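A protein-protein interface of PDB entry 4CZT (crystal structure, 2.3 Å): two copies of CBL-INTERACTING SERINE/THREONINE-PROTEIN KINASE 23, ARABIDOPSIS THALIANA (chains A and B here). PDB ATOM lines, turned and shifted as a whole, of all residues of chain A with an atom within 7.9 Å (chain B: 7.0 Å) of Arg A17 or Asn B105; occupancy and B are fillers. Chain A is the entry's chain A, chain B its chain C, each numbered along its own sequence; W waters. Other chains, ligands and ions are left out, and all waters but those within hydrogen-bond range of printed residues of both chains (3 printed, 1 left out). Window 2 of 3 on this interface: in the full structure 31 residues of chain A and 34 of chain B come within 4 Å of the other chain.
Printed residues of chain B within 4 Å of Arg A17: Asn B105. Asn B105 touches two residues of chain A. Ser B104 touches one residue of chain A. Of the printed residues of chain B, Leu A19 touches Ser B104 (3.2 Å), Asn B105 (3.5 Å) and Gly B106 (3.8 Å). Of the printed residues of chain B, Glu A21 touches Arg B107 (3.0 Å). Of the printed residues of chain B, Gly A168 touches Gly B106 (3.7 Å). Of the printed residues of chain A, Ile B102 touches Leu A169. Printed residues of chain A within 4 Å of Arg B107: Glu A21 (3.0 Å). Lys B109 touches none of the printed residues of chain A. The nearest residue of chain A that does not touch Asn B105 is Leu A169 (4.8 Å).
Water W3 lies within hydrogen-bond range of OE1 of Glu A21 (2.5 Å) and NH2 of Arg B107 (2.7 Å). Water W2 lies within hydrogen-bond range of the backbone carbonyl oxygen of Glu A21 (2.6 Å) and the guanidinium group of Arg B107 (2.9 Å). Water W1 lies within hydrogen-bond range of O of Gly A168 (2.7 Å), N of Arg B107 (2.9 Å) and N of Glu A21 (3.4 Å).
No position is printed for both chains. Of the 9 pairs that touch across the chains among the printed residues, none has its exchanged pair printed and touching as well.
Printed residues of chain A that touch a printed residue of chain B: Arg A17, Leu A19, Glu A21, Gly A168 and Leu A169. Hydrophobic or aromatic side chains of chain A within 4 Å of the printed part of chain B: Leu A19 and Leu A169. Among the printed residues, Asp or Glu carboxylates within 4 Å of a Lys or Arg side-chain nitrogen of the other chain: Glu A21 with Arg B107.
Among the printed residues, merely in contact across the chains: Leu A19 with Ser B104 (3.2 Å), Leu A19 with Gly B106 (3.8 Å), Gly A168 with Gly B106 (3.7 Å), Leu A169 with Ile B102 (3.7 Å), Leu A169 with Ser B103 (3.5 Å) and Leu A169 with Gly B106 (3.99 Å).
NH1 of Arg A17 is in hydrogen-bond range of OD1 of Asn B105 (3.3 Å). OE1 of Glu A21 lies within salt-bridge range of NH1 of Arg B107, at 3.0 Å. O of Asn B105 lies close to O of Leu A19.
The backbone carbonyl oxygen of Arg A17 sits at hydrogen-bond distance from the backbone NH of Phe A29, 3.0 Å away. The backbone NH (N) of Leu A19 is in hydrogen-bond range of the backbone carbonyl oxygen (O) of Val A27. The side-chain hydroxyl of Ser B104 sits at hydrogen-bond distance from the backbone carbonyl oxygen of Asp B100, 2.9 Å away.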
ATOM      1  N   ARG A   7     -30.920 -15.232 -14.226  1.00  0.00           N
ATOM      2  CA  ARG A   7     -31.446 -15.103 -15.584  1.00  0.00           C
ATOM      3  C   ARG A   7     -32.961 -15.319 -15.553  1.00  0.00           C
ATOM      4  O   ARG A   7     -33.471 -16.138 -14.784  1.00  0.00           O
ATOM      5  CB  ARG A   7     -30.799 -16.116 -16.537  1.00  0.00           C
ATOM      6  CG  ARG A   7     -29.314 -15.914 -16.824  1.00  0.00           C
ATOM      7  CD  ARG A   7     -28.802 -16.977 -17.803  1.00  0.00           C
ATOM      8  NE  ARG A   7     -27.396 -16.795 -18.158  1.00  0.00           N
ATOM      9  CZ  ARG A   7     -26.895 -17.008 -19.375  1.00  0.00           C
ATOM     10  NH1 ARG A   7     -27.686 -17.406 -20.366  1.00  0.00           N
ATOM     11  NH2 ARG A   7     -25.601 -16.817 -19.608  1.00  0.00           N
ATOM     12  N   GLU A  14     -34.505 -20.589 -20.769  1.00  0.00           N
ATOM     13  CA  GLU A  14     -33.847 -19.563 -20.001  1.00  0.00           C
ATOM     14  C   GLU A  14     -33.309 -18.513 -20.960  1.00  0.00           C
ATOM     15  O   GLU A  14     -32.576 -18.853 -21.891  1.00  0.00           O
ATOM     16  CB  GLU A  14     -32.732 -20.186 -19.189  1.00  0.00           C
ATOM     17  CG  GLU A  14     -32.038 -19.287 -18.220  1.00  0.00           C
ATOM     18  CD  GLU A  14     -31.166 -20.093 -17.283  1.00  0.00           C
ATOM     19  OE1 GLU A  14     -29.997 -20.380 -17.645  1.00  0.00           O
ATOM     20  OE2 GLU A  14     -31.668 -20.470 -16.202  1.00  0.00           O
ATOM     21  N   LEU A  15     -33.684 -17.251 -20.741  1.00  0.00           N
ATOM     22  CA  LEU A  15     -33.283 -16.153 -21.613  1.00  0.00           C
ATOM     23  C   LEU A  15     -31.908 -15.616 -21.282  1.00  0.00           C
ATOM     24  O   LEU A  15     -31.573 -15.383 -20.120  1.00  0.00           O
ATOM     25  CB  LEU A  15     -34.288 -15.006 -21.536  1.00  0.00           C
ATOM     26  CG  LEU A  15     -35.660 -15.268 -22.128  1.00  0.00           C
ATOM     27  CD1 LEU A  15     -36.526 -14.051 -21.938  1.00  0.00           C
ATOM     28  CD2 LEU A  15     -35.500 -15.553 -23.579  1.00  0.00           C
ATOM     29  N   GLY A  16     -31.117 -15.406 -22.323  1.00  0.00           N
ATOM     30  CA  GLY A  16     -29.789 -14.849 -22.175  1.00  0.00           C
ATOM     31  C   GLY A  16     -29.813 -13.426 -22.686  1.00  0.00           C
ATOM     32  O   GLY A  16     -30.788 -12.705 -22.469  1.00  0.00           O
ATOM     33  N   ARG A  17     -28.762 -13.018 -23.389  1.00  0.00           N
ATOM     34  CA  ARG A  17     -28.604 -11.610 -23.697  1.00  0.00           C
ATOM     35  C   ARG A  17     -29.340 -11.188 -24.978  1.00  0.00           C
ATOM     36  O   ARG A  17     -29.752 -12.017 -25.806  1.00  0.00           O
ATOM     37  CB  ARG A  17     -27.117 -11.248 -23.797  1.00  0.00           C
ATOM     38  CG  ARG A  17     -26.450 -11.666 -25.094  1.00  0.00           C
ATOM     39  CD  ARG A  17     -25.019 -11.129 -25.204  1.00  0.00           C
ATOM     40  NE  ARG A  17     -24.387 -11.617 -26.427  1.00  0.00           N
ATOM     41  CZ  ARG A  17     -24.214 -10.892 -27.529  1.00  0.00           C
ATOM     42  NH1 ARG A  17     -24.603  -9.622 -27.565  1.00  0.00           N
ATOM     43  NH2 ARG A  17     -23.645 -11.438 -28.595  1.00  0.00           N
ATOM     44  N   THR A  18     -29.491  -9.878 -25.104  1.00  0.00           N
ATOM     45  CA  THR A  18     -30.175  -9.251 -26.224  1.00  0.00           C
ATOM     46  C   THR A  18     -29.248  -9.104 -27.414  1.00  0.00           C
ATOM     47  O   THR A  18     -28.214  -8.445 -27.338  1.00  0.00           O
ATOM     48  CB  THR A  18     -30.721  -7.868 -25.827  1.00  0.00           C
ATOM     49  OG1 THR A  18     -31.546  -8.003 -24.663  1.00  0.00           O
ATOM     50  CG2 THR A  18     -31.525  -7.241 -26.954  1.00  0.00           C
ATOM     51  N   LEU A  19     -29.626  -9.738 -28.508  1.00  0.00           N
ATOM     52  CA  LEU A  19     -28.888  -9.657 -29.750  1.00  0.00           C
ATOM     53  C   LEU A  19     -29.280  -8.385 -30.512  1.00  0.00           C
ATOM     54  O   LEU A  19     -28.416  -7.645 -31.011  1.00  0.00           O
ATOM     55  CB  LEU A  19     -29.159 -10.902 -30.594  1.00  0.00           C
ATOM     56  CG  LEU A  19     -28.605 -10.971 -32.013  1.00  0.00           C
ATOM     57  CD1 LEU A  19     -27.113 -10.682 -31.990  1.00  0.00           C
ATOM     58  CD2 LEU A  19     -28.891 -12.334 -32.636  1.00  0.00           C
ATOM     59  N   GLY A  20     -30.587  -8.134 -30.591  1.00  0.00           N
ATOM     60  CA  GLY A  20     -31.102  -6.978 -31.299  1.00  0.00           C
ATOM     61  C   GLY A  20     -32.315  -6.354 -30.636  1.00  0.00           C
ATOM     62  O   GLY A  20     -33.155  -7.056 -30.071  1.00  0.00           O
ATOM     63  N   GLU A  21     -32.413  -5.030 -30.716  1.00  0.00           N
ATOM     64  CA  GLU A  21     -33.547  -4.316 -30.138  1.00  0.00           C
ATOM     65  C   GLU A  21     -34.192  -3.343 -31.136  1.00  0.00           C
ATOM     66  O   GLU A  21     -33.522  -2.457 -31.700  1.00  0.00           O
ATOM     67  CB  GLU A  21     -33.106  -3.565 -28.883  1.00  0.00           C
ATOM     68  CG  GLU A  21     -34.230  -2.865 -28.145  1.00  0.00           C
ATOM     69  CD  GLU A  21     -33.732  -1.917 -27.051  1.00  0.00           C
ATOM     70  OE1 GLU A  21     -32.511  -1.864 -26.788  1.00  0.00           O
ATOM     71  OE2 GLU A  21     -34.572  -1.214 -26.447  1.00  0.00           O
ATOM     72  N   LYS A  26     -37.745  -7.535 -29.537  1.00  0.00           N
ATOM     73  CA  LYS A  26     -36.359  -7.839 -29.192  1.00  0.00           C
ATOM     74  C   LYS A  26     -36.018  -9.260 -29.613  1.00  0.00           C
ATOM     75  O   LYS A  26     -36.890 -10.119 -29.694  1.00  0.00           O
ATOM     76  CB  LYS A  26     -36.112  -7.693 -27.694  1.00  0.00           C
ATOM     77  CG  LYS A  26     -35.845  -6.301 -27.219  1.00  0.00           C
ATOM     78  CD  LYS A  26     -35.661  -6.295 -25.707  1.00  0.00           C
ATOM     79  CE  LYS A  26     -35.551  -4.876 -25.149  1.00  0.00           C
ATOM     80  NZ  LYS A  26     -35.229  -4.924 -23.696  1.00  0.00           N
ATOM     81  N   VAL A  27     -34.744  -9.504 -29.873  1.00  0.00           N
ATOM     82  CA  VAL A  27     -34.275 -10.853 -30.127  1.00  0.00           C
ATOM     83  C   VAL A  27     -33.221 -11.204 -29.089  1.00  0.00           C
ATOM     84  O   VAL A  27     -32.238 -10.480 -28.919  1.00  0.00           O
ATOM     85  CB  VAL A  27     -33.713 -11.002 -31.536  1.00  0.00           C
ATOM     86  CG1 VAL A  27     -33.015 -12.347 -31.673  1.00  0.00           C
ATOM     87  CG2 VAL A  27     -34.833 -10.871 -32.558  1.00  0.00           C
ATOM     88  N   LYS A  28     -33.463 -12.290 -28.363  1.00  0.00           N
ATOM     89  CA  LYS A  28     -32.539 -12.741 -27.325  1.00  0.00           C
ATOM     90  C   LYS A  28     -32.063 -14.146 -27.588  1.00  0.00           C
ATOM     91  O   LYS A  28     -32.754 -14.942 -28.233  1.00  0.00           O
ATOM     92  CB  LYS A  28     -33.193 -12.691 -25.959  1.00  0.00           C
ATOM     93  CG  LYS A  28     -33.627 -11.313 -25.586  1.00  0.00           C
ATOM     94  CD  LYS A  28     -34.215 -11.281 -24.211  1.00  0.00           C
ATOM     95  CE  LYS A  28     -34.505  -9.847 -23.810  1.00  0.00           C
ATOM     96  NZ  LYS A  28     -34.743  -9.780 -22.362  1.00  0.00           N
ATOM     97  N   PHE A  29     -30.875 -14.450 -27.091  1.00  0.00           N
ATOM     98  CA  PHE A  29     -30.429 -15.833 -27.054  1.00  0.00           C
ATOM     99  C   PHE A  29     -31.192 -16.516 -25.957  1.00  0.00           C
ATOM    100  O   PHE A  29     -31.540 -15.885 -24.963  1.00  0.00           O
ATOM    101  CB  PHE A  29     -28.927 -15.950 -26.782  1.00  0.00           C
ATOM    102  CG  PHE A  29     -28.077 -15.450 -27.891  1.00  0.00           C
ATOM    103  CD1 PHE A  29     -27.719 -16.288 -28.931  1.00  0.00           C
ATOM    104  CD2 PHE A  29     -27.623 -14.139 -27.894  1.00  0.00           C
ATOM    105  CE1 PHE A  29     -26.928 -15.826 -29.964  1.00  0.00           C
ATOM    106  CE2 PHE A  29     -26.835 -13.669 -28.924  1.00  0.00           C
ATOM    107  CZ  PHE A  29     -26.486 -14.516 -29.962  1.00  0.00           C
ATOM    108  N   ALA A  30     -31.441 -17.808 -26.120  1.00  0.00           N
ATOM    109  CA  ALA A  30     -32.038 -18.554 -25.037  1.00  0.00           C
ATOM    110  C   ALA A  30     -31.627 -19.998 -25.103  1.00  0.00           C
ATOM    111  O   ALA A  30     -31.076 -20.468 -26.105  1.00  0.00           O
ATOM    112  CB  ALA A  30     -33.565 -18.436 -25.060  1.00  0.00           C
ATOM    113  N   VAL A  39     -31.523 -21.539 -28.841  1.00  0.00           N
ATOM    114  CA  VAL A  39     -32.539 -21.015 -29.728  1.00  0.00           C
ATOM    115  C   VAL A  39     -32.484 -19.500 -29.723  1.00  0.00           C
ATOM    116  O   VAL A  39     -31.793 -18.897 -28.918  1.00  0.00           O
ATOM    117  CB  VAL A  39     -33.957 -21.466 -29.310  1.00  0.00           C
ATOM    118  CG1 VAL A  39     -34.153 -22.985 -29.498  1.00  0.00           C
ATOM    119  CG2 VAL A  39     -34.237 -21.036 -27.880  1.00  0.00           C
ATOM    120  N   ILE A  41     -35.043 -16.258 -29.237  1.00  0.00           N
ATOM    121  CA  ILE A  41     -36.414 -15.929 -28.909  1.00  0.00           C
ATOM    122  C   ILE A  41     -36.740 -14.482 -29.282  1.00  0.00           C
ATOM    123  O   ILE A  41     -36.049 -13.541 -28.882  1.00  0.00           O
ATOM    124  CB  ILE A  41     -36.716 -16.179 -27.426  1.00  0.00           C
ATOM    125  CG1 ILE A  41     -36.654 -17.685 -27.145  1.00  0.00           C
ATOM    126  CG2 ILE A  41     -38.101 -15.669 -27.082  1.00  0.00           C
ATOM    127  CD1 ILE A  41     -37.103 -18.061 -25.736  1.00  0.00           C
ATOM    128  N   GLY A 168     -34.175  -4.578 -34.902  1.00  0.00           N
ATOM    129  CA  GLY A 168     -32.904  -3.879 -34.919  1.00  0.00           C
ATOM    130  C   GLY A 168     -31.736  -4.722 -35.370  1.00  0.00           C
ATOM    131  O   GLY A 168     -30.650  -4.608 -34.830  1.00  0.00           O
ATOM    132  N   LEU A 169     -31.963  -5.564 -36.366  1.00  0.00           N
ATOM    133  CA  LEU A 169     -30.935  -6.461 -36.873  1.00  0.00           C
ATOM    134  C   LEU A 169     -30.807  -6.364 -38.386  1.00  0.00           C
ATOM    135  O   LEU A 169     -30.025  -7.087 -38.975  1.00  0.00           O
ATOM    136  CB  LEU A 169     -31.243  -7.917 -36.481  1.00  0.00           C
ATOM    137  CG  LEU A 169     -30.896  -8.293 -35.039  1.00  0.00           C
ATOM    138  CD1 LEU A 169     -31.567  -9.605 -34.612  1.00  0.00           C
ATOM    139  CD2 LEU A 169     -29.385  -8.379 -34.903  1.00  0.00           C
ATOM    140  N   ASP B 100     -22.283  -5.278 -41.742  1.00  0.00           N
ATOM    141  CA  ASP B 100     -22.138  -6.621 -41.166  1.00  0.00           C
ATOM    142  C   ASP B 100     -22.162  -6.601 -39.639  1.00  0.00           C
ATOM    143  O   ASP B 100     -22.672  -7.522 -39.008  1.00  0.00           O
ATOM    144  CB  ASP B 100     -20.840  -7.272 -41.631  1.00  0.00           C
ATOM    145  CG  ASP B 100     -21.038  -8.171 -42.816  1.00  0.00           C
ATOM    146  OD1 ASP B 100     -21.997  -7.934 -43.587  1.00  0.00           O
ATOM    147  OD2 ASP B 100     -20.229  -9.110 -42.985  1.00  0.00           O
ATOM    148  N   LYS B 101     -21.611  -5.541 -39.055  1.00  0.00           N
ATOM    149  CA  LYS B 101     -21.592  -5.388 -37.606  1.00  0.00           C
ATOM    150  C   LYS B 101     -22.991  -5.291 -37.000  1.00  0.00           C
ATOM    151  O   LYS B 101     -23.205  -5.639 -35.840  1.00  0.00           O
ATOM    152  CB  LYS B 101     -20.796  -4.148 -37.214  1.00  0.00           C
ATOM    153  CG  LYS B 101     -19.327  -4.247 -37.512  1.00  0.00           C
ATOM    154  CD  LYS B 101     -18.577  -3.069 -36.915  1.00  0.00           C
ATOM    155  CE  LYS B 101     -17.065  -3.254 -37.065  1.00  0.00           C
ATOM    156  NZ  LYS B 101     -16.306  -2.261 -36.242  1.00  0.00           N
ATOM    157  N   ILE B 102     -23.937  -4.798 -37.783  1.00  0.00           N
ATOM    158  CA  ILE B 102     -25.293  -4.628 -37.301  1.00  0.00           C
ATOM    159  C   ILE B 102     -26.053  -5.937 -37.375  1.00  0.00           C
ATOM    160  O   ILE B 102     -26.679  -6.351 -36.394  1.00  0.00           O
ATOM    161  CB  ILE B 102     -26.030  -3.546 -38.101  1.00  0.00           C
ATOM    162  CG1 ILE B 102     -25.383  -2.188 -37.835  1.00  0.00           C
ATOM    163  CG2 ILE B 102     -27.503  -3.533 -37.735  1.00  0.00           C
ATOM    164  CD1 ILE B 102     -25.906  -1.106 -38.715  1.00  0.00           C
ATOM    165  N   SER B 103     -25.969  -6.595 -38.530  1.00  0.00           N
ATOM    166  CA  SER B 103     -26.620  -7.887 -38.757  1.00  0.00           C
ATOM    167  C   SER B 103     -26.252  -8.964 -37.736  1.00  0.00           C
ATOM    168  O   SER B 103     -27.001  -9.924 -37.543  1.00  0.00           O
ATOM    169  CB  SER B 103     -26.276  -8.408 -40.149  1.00  0.00           C
ATOM    170  OG  SER B 103     -26.477  -7.411 -41.120  1.00  0.00           O
ATOM    171  N   SER B 104     -25.099  -8.808 -37.094  1.00  0.00           N
ATOM    172  CA  SER B 104     -24.557  -9.866 -36.256  1.00  0.00           C
ATOM    173  C   SER B 104     -24.533  -9.502 -34.766  1.00  0.00           C
ATOM    174  O   SER B 104     -24.527 -10.386 -33.905  1.00  0.00           O
ATOM    175  CB  SER B 104     -23.146 -10.248 -36.744  1.00  0.00           C
ATOM    176  OG  SER B 104     -22.241  -9.158 -36.673  1.00  0.00           O
ATOM    177  N   ASN B 105     -24.520  -8.212 -34.452  1.00  0.00           N
ATOM    178  CA  ASN B 105     -24.529  -7.799 -33.053  1.00  0.00           C
ATOM    179  C   ASN B 105     -25.432  -6.598 -32.777  1.00  0.00           C
ATOM    180  O   ASN B 105     -25.400  -6.019 -31.689  1.00  0.00           O
ATOM    181  CB  ASN B 105     -23.110  -7.480 -32.575  1.00  0.00           C
ATOM    182  CG  ASN B 105     -22.997  -7.494 -31.052  1.00  0.00           C
ATOM    183  OD1 ASN B 105     -23.490  -8.416 -30.394  1.00  0.00           O
ATOM    184  ND2 ASN B 105     -22.385  -6.449 -30.484  1.00  0.00           N
ATOM    185  N   GLY B 106     -26.239  -6.212 -33.760  1.00  0.00           N
ATOM    186  CA  GLY B 106     -27.173  -5.121 -33.544  1.00  0.00           C
ATOM    187  C   GLY B 106     -26.520  -3.758 -33.590  1.00  0.00           C
ATOM    188  O   GLY B 106     -25.444  -3.587 -34.160  1.00  0.00           O
ATOM    189  N   ARG B 107     -27.181  -2.770 -32.998  1.00  0.00           N
ATOM    190  CA  ARG B 107     -26.740  -1.396 -33.145  1.00  0.00           C
ATOM    191  C   ARG B 107     -25.341  -1.200 -32.566  1.00  0.00           C
ATOM    192  O   ARG B 107     -24.965  -1.870 -31.603  1.00  0.00           O
ATOM    193  CB  ARG B 107     -27.739  -0.439 -32.481  1.00  0.00           C
ATOM    194  CG  ARG B 107     -27.799  -0.499 -30.958  1.00  0.00           C
ATOM    195  CD  ARG B 107     -28.708   0.595 -30.460  1.00  0.00           C
ATOM    196  NE  ARG B 107     -28.772   0.700 -29.006  1.00  0.00           N
ATOM    197  CZ  ARG B 107     -29.707   0.119 -28.256  1.00  0.00           C
ATOM    198  NH1 ARG B 107     -30.654  -0.629 -28.814  1.00  0.00           N
ATOM    199  NH2 ARG B 107     -29.692   0.284 -26.943  1.00  0.00           N
ATOM    200  N   LEU B 108     -24.569  -0.293 -33.163  1.00  0.00           N
ATOM    201  CA  LEU B 108     -23.258   0.067 -32.625  1.00  0.00           C
ATOM    202  C   LEU B 108     -23.422   0.998 -31.438  1.00  0.00           C
ATOM    203  O   LEU B 108     -24.459   1.654 -31.295  1.00  0.00           O
ATOM    204  CB  LEU B 108     -22.380   0.742 -33.681  1.00  0.00           C
ATOM    205  CG  LEU B 108     -22.277   0.143 -35.085  1.00  0.00           C
ATOM    206  CD1 LEU B 108     -21.169   0.859 -35.828  1.00  0.00           C
ATOM    207  CD2 LEU B 108     -22.029  -1.346 -35.054  1.00  0.00           C
ATOM    208  N   LYS B 109     -22.409   1.067 -30.581  1.00  0.00           N
ATOM    209  CA  LYS B 109     -22.439   2.028 -29.482  1.00  0.00           C
ATOM    210  C   LYS B 109     -22.229   3.416 -30.058  1.00  0.00           C
ATOM    211  O   LYS B 109     -21.662   3.542 -31.146  1.00  0.00           O
ATOM    212  CB  LYS B 109     -21.383   1.703 -28.422  1.00  0.00           C
ATOM    213  CG  LYS B 109     -21.212   0.208 -28.138  1.00  0.00           C
ATOM    214  CD  LYS B 109     -20.194  -0.054 -27.030  1.00  0.00           C
ATOM    215  CE  LYS B 109     -19.399  -1.330 -27.297  1.00  0.00           C
ATOM    216  NZ  LYS B 109     -19.793  -2.463 -26.401  1.00  0.00           N
HETATM  217  O   HOH W   1     -30.011  -3.419 -32.477  1.00  0.00           O
HETATM  218  O   HOH W   2     -31.300  -1.155 -31.620  1.00  0.00           O
HETATM  219  O   HOH W   3     -31.760  -0.016 -25.212  1.00  0.00           O
